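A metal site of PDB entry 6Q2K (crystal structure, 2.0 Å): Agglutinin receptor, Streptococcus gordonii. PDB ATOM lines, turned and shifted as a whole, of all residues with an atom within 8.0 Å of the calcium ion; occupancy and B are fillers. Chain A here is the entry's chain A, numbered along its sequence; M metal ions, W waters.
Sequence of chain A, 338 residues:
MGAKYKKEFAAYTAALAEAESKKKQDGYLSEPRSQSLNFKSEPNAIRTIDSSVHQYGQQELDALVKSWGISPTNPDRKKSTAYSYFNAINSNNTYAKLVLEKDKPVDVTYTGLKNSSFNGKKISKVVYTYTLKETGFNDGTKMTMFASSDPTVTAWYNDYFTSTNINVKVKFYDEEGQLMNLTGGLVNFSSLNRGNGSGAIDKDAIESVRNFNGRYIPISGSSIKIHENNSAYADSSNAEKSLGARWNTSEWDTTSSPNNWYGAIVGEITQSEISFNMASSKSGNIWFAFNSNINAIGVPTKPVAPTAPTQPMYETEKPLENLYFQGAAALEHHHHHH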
ATOM      1  N   TRP A 156      27.725 -15.154  27.736  1.00  0.00           N
ATOM      2  CA  TRP A 156      27.178 -14.364  26.634  1.00  0.00           C
ATOM      3  C   TRP A 156      26.731 -15.341  25.550  1.00  0.00           C
ATOM      4  O   TRP A 156      27.369 -16.364  25.347  1.00  0.00           O
ATOM      5  CB  TRP A 156      28.217 -13.434  26.025  1.00  0.00           C
ATOM      6  CG  TRP A 156      28.637 -12.310  26.891  1.00  0.00           C
ATOM      7  CD1 TRP A 156      29.489 -12.375  27.941  1.00  0.00           C
ATOM      8  CD2 TRP A 156      28.264 -10.931  26.764  1.00  0.00           C
ATOM      9  NE1 TRP A 156      29.664 -11.128  28.495  1.00  0.00           N
ATOM     10  CE2 TRP A 156      28.919 -10.222  27.777  1.00  0.00           C
ATOM     11  CE3 TRP A 156      27.429 -10.226  25.878  1.00  0.00           C
ATOM     12  CZ2 TRP A 156      28.776  -8.836  27.956  1.00  0.00           C
ATOM     13  CZ3 TRP A 156      27.285  -8.848  26.045  1.00  0.00           C
ATOM     14  CH2 TRP A 156      27.953  -8.171  27.080  1.00  0.00           C
ATOM     15  N   SER A 190      18.134 -10.781  35.872  1.00  0.00           N
ATOM     16  CA  SER A 190      18.280  -9.338  35.715  1.00  0.00           C
ATOM     17  C   SER A 190      18.421  -8.955  34.253  1.00  0.00           C
ATOM     18  O   SER A 190      18.550  -9.814  33.374  1.00  0.00           O
ATOM     19  CB  SER A 190      19.518  -8.858  36.472  1.00  0.00           C
ATOM     20  OG  SER A 190      20.684  -9.520  35.996  1.00  0.00           O
ATOM     21  N   SER A 191      18.399  -7.648  34.015  1.00  0.00           N
ATOM     22  CA  SER A 191      18.797  -7.065  32.734  1.00  0.00           C
ATOM     23  C   SER A 191      18.062  -7.722  31.561  1.00  0.00           C
ATOM     24  O   SER A 191      18.679  -8.142  30.586  1.00  0.00           O
ATOM     25  CB  SER A 191      20.318  -7.165  32.591  1.00  0.00           C
ATOM     26  OG  SER A 191      20.776  -6.466  31.446  1.00  0.00           O
ATOM     27  N   LEU A 192      16.736  -7.827  31.677  1.00  0.00           N
ATOM     28  CA  LEU A 192      15.897  -8.393  30.628  1.00  0.00           C
ATOM     29  C   LEU A 192      15.343  -7.233  29.795  1.00  0.00           C
ATOM     30  O   LEU A 192      14.180  -6.835  29.935  1.00  0.00           O
ATOM     31  CB  LEU A 192      14.791  -9.264  31.230  1.00  0.00           C
ATOM     32  CG  LEU A 192      15.292 -10.496  32.008  1.00  0.00           C
ATOM     33  CD1 LEU A 192      14.140 -11.217  32.691  1.00  0.00           C
ATOM     34  CD2 LEU A 192      16.048 -11.452  31.097  1.00  0.00           C
ATOM     35  N   ASN A 193      16.215  -6.705  28.938  1.00  0.00           N
ATOM     36  CA  ASN A 193      15.941  -5.498  28.174  1.00  0.00           C
ATOM     37  C   ASN A 193      14.910  -5.768  27.093  1.00  0.00           C
ATOM     38  O   ASN A 193      14.872  -6.854  26.508  1.00  0.00           O
ATOM     39  CB  ASN A 193      17.203  -4.943  27.518  1.00  0.00           C
ATOM     40  CG  ASN A 193      18.293  -4.618  28.532  1.00  0.00           C
ATOM     41  OD1 ASN A 193      18.998  -5.511  28.991  1.00  0.00           O
ATOM     42  ND2 ASN A 193      18.449  -3.338  28.862  1.00  0.00           N
ATOM     43  N   ARG A 194      14.060  -4.774  26.853  1.00  0.00           N
ATOM     44  CA  ARG A 194      13.183  -4.723  25.684  1.00  0.00           C
ATOM     45  C   ARG A 194      13.281  -3.322  25.097  1.00  0.00           C
ATOM     46  O   ARG A 194      13.307  -2.336  25.827  1.00  0.00           O
ATOM     47  CB  ARG A 194      11.732  -5.052  26.034  1.00  0.00           C
ATOM     48  CG  ARG A 194      10.816  -4.987  24.816  1.00  0.00           C
ATOM     49  CD  ARG A 194       9.559  -5.825  24.974  1.00  0.00           C
ATOM     50  NE  ARG A 194       8.841  -5.917  23.703  1.00  0.00           N
ATOM     51  CZ  ARG A 194       7.773  -6.680  23.481  1.00  0.00           C
ATOM     52  NH1 ARG A 194       7.250  -7.449  24.431  1.00  0.00           N
ATOM     53  NH2 ARG A 194       7.218  -6.683  22.264  1.00  0.00           N
ATOM     54  N   ASN A 196      15.904  -2.210  23.427  1.00  0.00           N
ATOM     55  CA  ASN A 196      17.303  -1.768  23.521  1.00  0.00           C
ATOM     56  C   ASN A 196      18.119  -2.219  22.303  1.00  0.00           C
ATOM     57  O   ASN A 196      19.341  -2.342  22.385  1.00  0.00           O
ATOM     58  CB  ASN A 196      17.924  -2.321  24.818  1.00  0.00           C
ATOM     59  CG  ASN A 196      19.173  -1.561  25.247  1.00  0.00           C
ATOM     60  OD1 ASN A 196      19.149  -0.352  25.450  1.00  0.00           O
ATOM     61  ND2 ASN A 196      20.274  -2.294  25.403  1.00  0.00           N
ATOM     62  N   GLU A 207      15.020  -9.486  25.310  1.00  0.00           N
ATOM     63  CA  GLU A 207      15.738 -10.503  26.086  1.00  0.00           C
ATOM     64  C   GLU A 207      14.767 -11.069  27.116  1.00  0.00           C
ATOM     65  O   GLU A 207      14.006 -10.309  27.740  1.00  0.00           O
ATOM     66  CB  GLU A 207      16.955  -9.912  26.775  1.00  0.00           C
ATOM     67  CG  GLU A 207      18.010  -9.373  25.806  1.00  0.00           C
ATOM     68  CD  GLU A 207      19.080  -8.549  26.495  1.00  0.00           C
ATOM     69  OE1 GLU A 207      19.420  -8.850  27.655  1.00  0.00           O
ATOM     70  OE2 GLU A 207      19.576  -7.600  25.866  1.00  0.00           O
ATOM     71  N   SER A 208      14.799 -12.377  27.310  1.00  0.00           N
ATOM     72  CA  SER A 208      13.844 -13.048  28.193  1.00  0.00           C
ATOM     73  C   SER A 208      14.411 -14.300  28.845  1.00  0.00           C
ATOM     74  O   SER A 208      15.433 -14.843  28.425  1.00  0.00           O
ATOM     75  CB  SER A 208      12.579 -13.412  27.399  1.00  0.00           C
ATOM     76  OG  SER A 208      12.841 -14.399  26.419  1.00  0.00           O
ATOM     77  N   THR A 249      17.577   3.055  29.448  1.00  0.00           N
ATOM     78  CA  THR A 249      18.461   1.908  29.743  1.00  0.00           C
ATOM     79  C   THR A 249      19.639   2.276  30.653  1.00  0.00           C
ATOM     80  O   THR A 249      19.832   1.657  31.695  1.00  0.00           O
ATOM     81  CB  THR A 249      18.996   1.269  28.454  1.00  0.00           C
ATOM     82  OG1 THR A 249      17.896   0.745  27.700  1.00  0.00           O
ATOM     83  CG2 THR A 249      19.976   0.120  28.745  1.00  0.00           C
ATOM     84  N   TRP A 252      19.071   2.593  34.541  1.00  0.00           N
ATOM     85  CA  TRP A 252      18.747   1.410  35.361  1.00  0.00           C
ATOM     86  C   TRP A 252      19.633   0.166  35.153  1.00  0.00           C
ATOM     87  O   TRP A 252      19.914  -0.541  36.124  1.00  0.00           O
ATOM     88  CB  TRP A 252      17.269   1.032  35.221  1.00  0.00           C
ATOM     89  CG  TRP A 252      16.836   0.449  33.901  1.00  0.00           C
ATOM     90  CD1 TRP A 252      16.233   1.117  32.878  1.00  0.00           C
ATOM     91  CD2 TRP A 252      16.935  -0.914  33.482  1.00  0.00           C
ATOM     92  NE1 TRP A 252      15.970   0.259  31.840  1.00  0.00           N
ATOM     93  CE2 TRP A 252      16.386  -0.996  32.181  1.00  0.00           C
ATOM     94  CE3 TRP A 252      17.439  -2.085  34.083  1.00  0.00           C
ATOM     95  CZ2 TRP A 252      16.342  -2.200  31.462  1.00  0.00           C
ATOM     96  CZ3 TRP A 252      17.399  -3.275  33.363  1.00  0.00           C
ATOM     97  CH2 TRP A 252      16.842  -3.326  32.058  1.00  0.00           C
ATOM     98  N   ASP A 253      20.063  -0.104  33.927  1.00  0.00           N
ATOM     99  CA  ASP A 253      20.654  -1.407  33.564  1.00  0.00           C
ATOM    100  C   ASP A 253      22.141  -1.538  33.907  1.00  0.00           C
ATOM    101  O   ASP A 253      23.000  -1.637  33.016  1.00  0.00           O
ATOM    102  CB  ASP A 253      20.386  -1.697  32.069  1.00  0.00           C
ATOM    103  CG  ASP A 253      20.733  -3.115  31.665  1.00  0.00           C
ATOM    104  OD1 ASP A 253      20.867  -3.995  32.544  1.00  0.00           O
ATOM    105  OD2 ASP A 253      20.870  -3.353  30.437  1.00  0.00           O
ATOM    106  N   GLY A 263      14.257  -3.754  35.418  1.00  0.00           N
ATOM    107  CA  GLY A 263      14.364  -4.787  34.387  1.00  0.00           C
ATOM    108  C   GLY A 263      14.638  -6.178  34.916  1.00  0.00           C
ATOM    109  O   GLY A 263      15.212  -7.002  34.197  1.00  0.00           O
ATOM    110  N   SER A 283      19.051  -8.917  19.192  1.00  0.00           N
ATOM    111  CA  SER A 283      19.930  -8.296  20.187  1.00  0.00           C
ATOM    112  C   SER A 283      21.428  -8.345  19.852  1.00  0.00           C
ATOM    113  O   SER A 283      22.189  -7.533  20.370  1.00  0.00           O
ATOM    114  CB  SER A 283      19.689  -8.933  21.557  1.00  0.00           C
ATOM    115  OG  SER A 283      18.337  -8.768  21.938  1.00  0.00           O
ATOM    116  N   ASN A 285      24.417  -9.432  20.740  1.00  0.00           N
ATOM    117  CA  ASN A 285      25.100  -9.972  21.923  1.00  0.00           C
ATOM    118  C   ASN A 285      24.136  -9.921  23.091  1.00  0.00           C
ATOM    119  O   ASN A 285      23.437  -8.926  23.270  1.00  0.00           O
ATOM    120  CB  ASN A 285      26.318  -9.113  22.292  1.00  0.00           C
ATOM    121  CG  ASN A 285      27.499  -9.303  21.354  1.00  0.00           C
ATOM    122  OD1 ASN A 285      27.494 -10.177  20.496  1.00  0.00           O
ATOM    123  ND2 ASN A 285      28.514  -8.470  21.524  1.00  0.00           N
ATOM    124  N   ILE A 286      24.112 -10.984  23.888  1.00  0.00           N
ATOM    125  CA  ILE A 286      23.245 -11.067  25.062  1.00  0.00           C
ATOM    126  C   ILE A 286      24.057 -11.627  26.233  1.00  0.00           C
ATOM    127  O   ILE A 286      24.457 -12.787  26.197  1.00  0.00           O
ATOM    128  CB  ILE A 286      22.011 -11.980  24.831  1.00  0.00           C
ATOM    129  CG1 ILE A 286      21.260 -11.570  23.551  1.00  0.00           C
ATOM    130  CG2 ILE A 286      21.080 -11.927  26.037  1.00  0.00           C
ATOM    131  CD1 ILE A 286      21.705 -12.274  22.295  1.00  0.00           C
ATOM    132  N   TRP A 287      24.291 -10.795  27.231  1.00  0.00           N
ATOM    133  CA  TRP A 287      24.902 -11.215  28.485  1.00  0.00           C
ATOM    134  C   TRP A 287      23.795 -11.770  29.367  1.00  0.00           C
ATOM    135  O   TRP A 287      22.789 -11.114  29.589  1.00  0.00           O
ATOM    136  CB  TRP A 287      25.587 -10.023  29.178  1.00  0.00           C
ATOM    137  CG  TRP A 287      26.212 -10.310  30.526  1.00  0.00           C
ATOM    138  CD1 TRP A 287      26.579 -11.523  31.036  1.00  0.00           C
ATOM    139  CD2 TRP A 287      26.544  -9.337  31.523  1.00  0.00           C
ATOM    140  NE1 TRP A 287      27.109 -11.372  32.298  1.00  0.00           N
ATOM    141  CE2 TRP A 287      27.100 -10.042  32.614  1.00  0.00           C
ATOM    142  CE3 TRP A 287      26.423  -7.947  31.600  1.00  0.00           C
ATOM    143  CZ2 TRP A 287      27.535  -9.395  33.783  1.00  0.00           C
ATOM    144  CZ3 TRP A 287      26.864  -7.302  32.760  1.00  0.00           C
ATOM    145  CH2 TRP A 287      27.404  -8.027  33.832  1.00  0.00           C
ATOM    146  N   PHE A 288      23.964 -13.009  29.826  1.00  0.00           N
ATOM    147  CA  PHE A 288      23.037 -13.614  30.772  1.00  0.00           C
ATOM    148  C   PHE A 288      23.804 -14.039  32.018  1.00  0.00           C
ATOM    149  O   PHE A 288      24.504 -15.047  31.989  1.00  0.00           O
ATOM    150  CB  PHE A 288      22.317 -14.802  30.144  1.00  0.00           C
ATOM    151  CG  PHE A 288      21.079 -15.213  30.885  1.00  0.00           C
ATOM    152  CD1 PHE A 288      21.156 -15.975  32.048  1.00  0.00           C
ATOM    153  CD2 PHE A 288      19.829 -14.834  30.427  1.00  0.00           C
ATOM    154  CE1 PHE A 288      20.015 -16.340  32.743  1.00  0.00           C
ATOM    155  CE2 PHE A 288      18.677 -15.197  31.113  1.00  0.00           C
ATOM    156  CZ  PHE A 288      18.765 -15.949  32.266  1.00  0.00           C
ATOM    157  N   ALA A 289      23.678 -13.257  33.085  1.00  0.00           N
ATOM    158  CA  ALA A 289      24.309 -13.582  34.373  1.00  0.00           C
ATOM    159  C   ALA A 289      23.314 -14.331  35.240  1.00  0.00           C
ATOM    160  O   ALA A 289      22.164 -13.917  35.359  1.00  0.00           O
ATOM    161  CB  ALA A 289      24.762 -12.317  35.069  1.00  0.00           C
ATOM    162  N   GLU A 332      28.926  -4.123  27.322  1.00  0.00           N
ATOM    163  CA  GLU A 332      27.542  -3.743  27.022  1.00  0.00           C
ATOM    164  C   GLU A 332      27.445  -2.474  26.187  1.00  0.00           C
ATOM    165  O   GLU A 332      28.140  -1.492  26.450  1.00  0.00           O
ATOM    166  CB  GLU A 332      26.743  -3.549  28.319  1.00  0.00           C
ATOM    167  CG  GLU A 332      26.496  -4.828  29.101  1.00  0.00           C
ATOM    168  CD  GLU A 332      25.240  -5.556  28.667  1.00  0.00           C
ATOM    169  OE1 GLU A 332      25.105  -5.862  27.465  1.00  0.00           O
ATOM    170  OE2 GLU A 332      24.390  -5.830  29.529  1.00  0.00           O
HETATM  171 CA    CA M   1      20.533  -7.305  29.273  1.00  0.00          CA
HETATM  172  O   HOH W   1      22.318  -8.669  29.383  1.00  0.00           O
HETATM  173  O   HOH W   2      21.858  -5.408  28.720  1.00  0.00           O
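OD2 of Asp 253 is in hydrogen-bond range of ND2 of Asn 193, 2.9 Å away. The side-chain carboxylate (OD1) of Asp 253 sits close to the side-chain hydroxyl (OG) of Ser 191, at 2.7 Å. The backbone NH (N) of Ser 191 lies within hydrogen-bond range of the backbone carbonyl oxygen (O) of Gly 263 (3.3 Å).
Within 4 Å of the calcium ion: Ser 191, Asn 193 and Glu 207.
The calcium ion is bound by water W1, OG of Ser 191, OD1 of Asn 193, water W2, O of Ser 191 and OE1 of Glu 207. The calcium ion has six donor atoms within binding distance.
Water W2 bridges OE2 of Glu 332 and OD2 of Asp 253.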
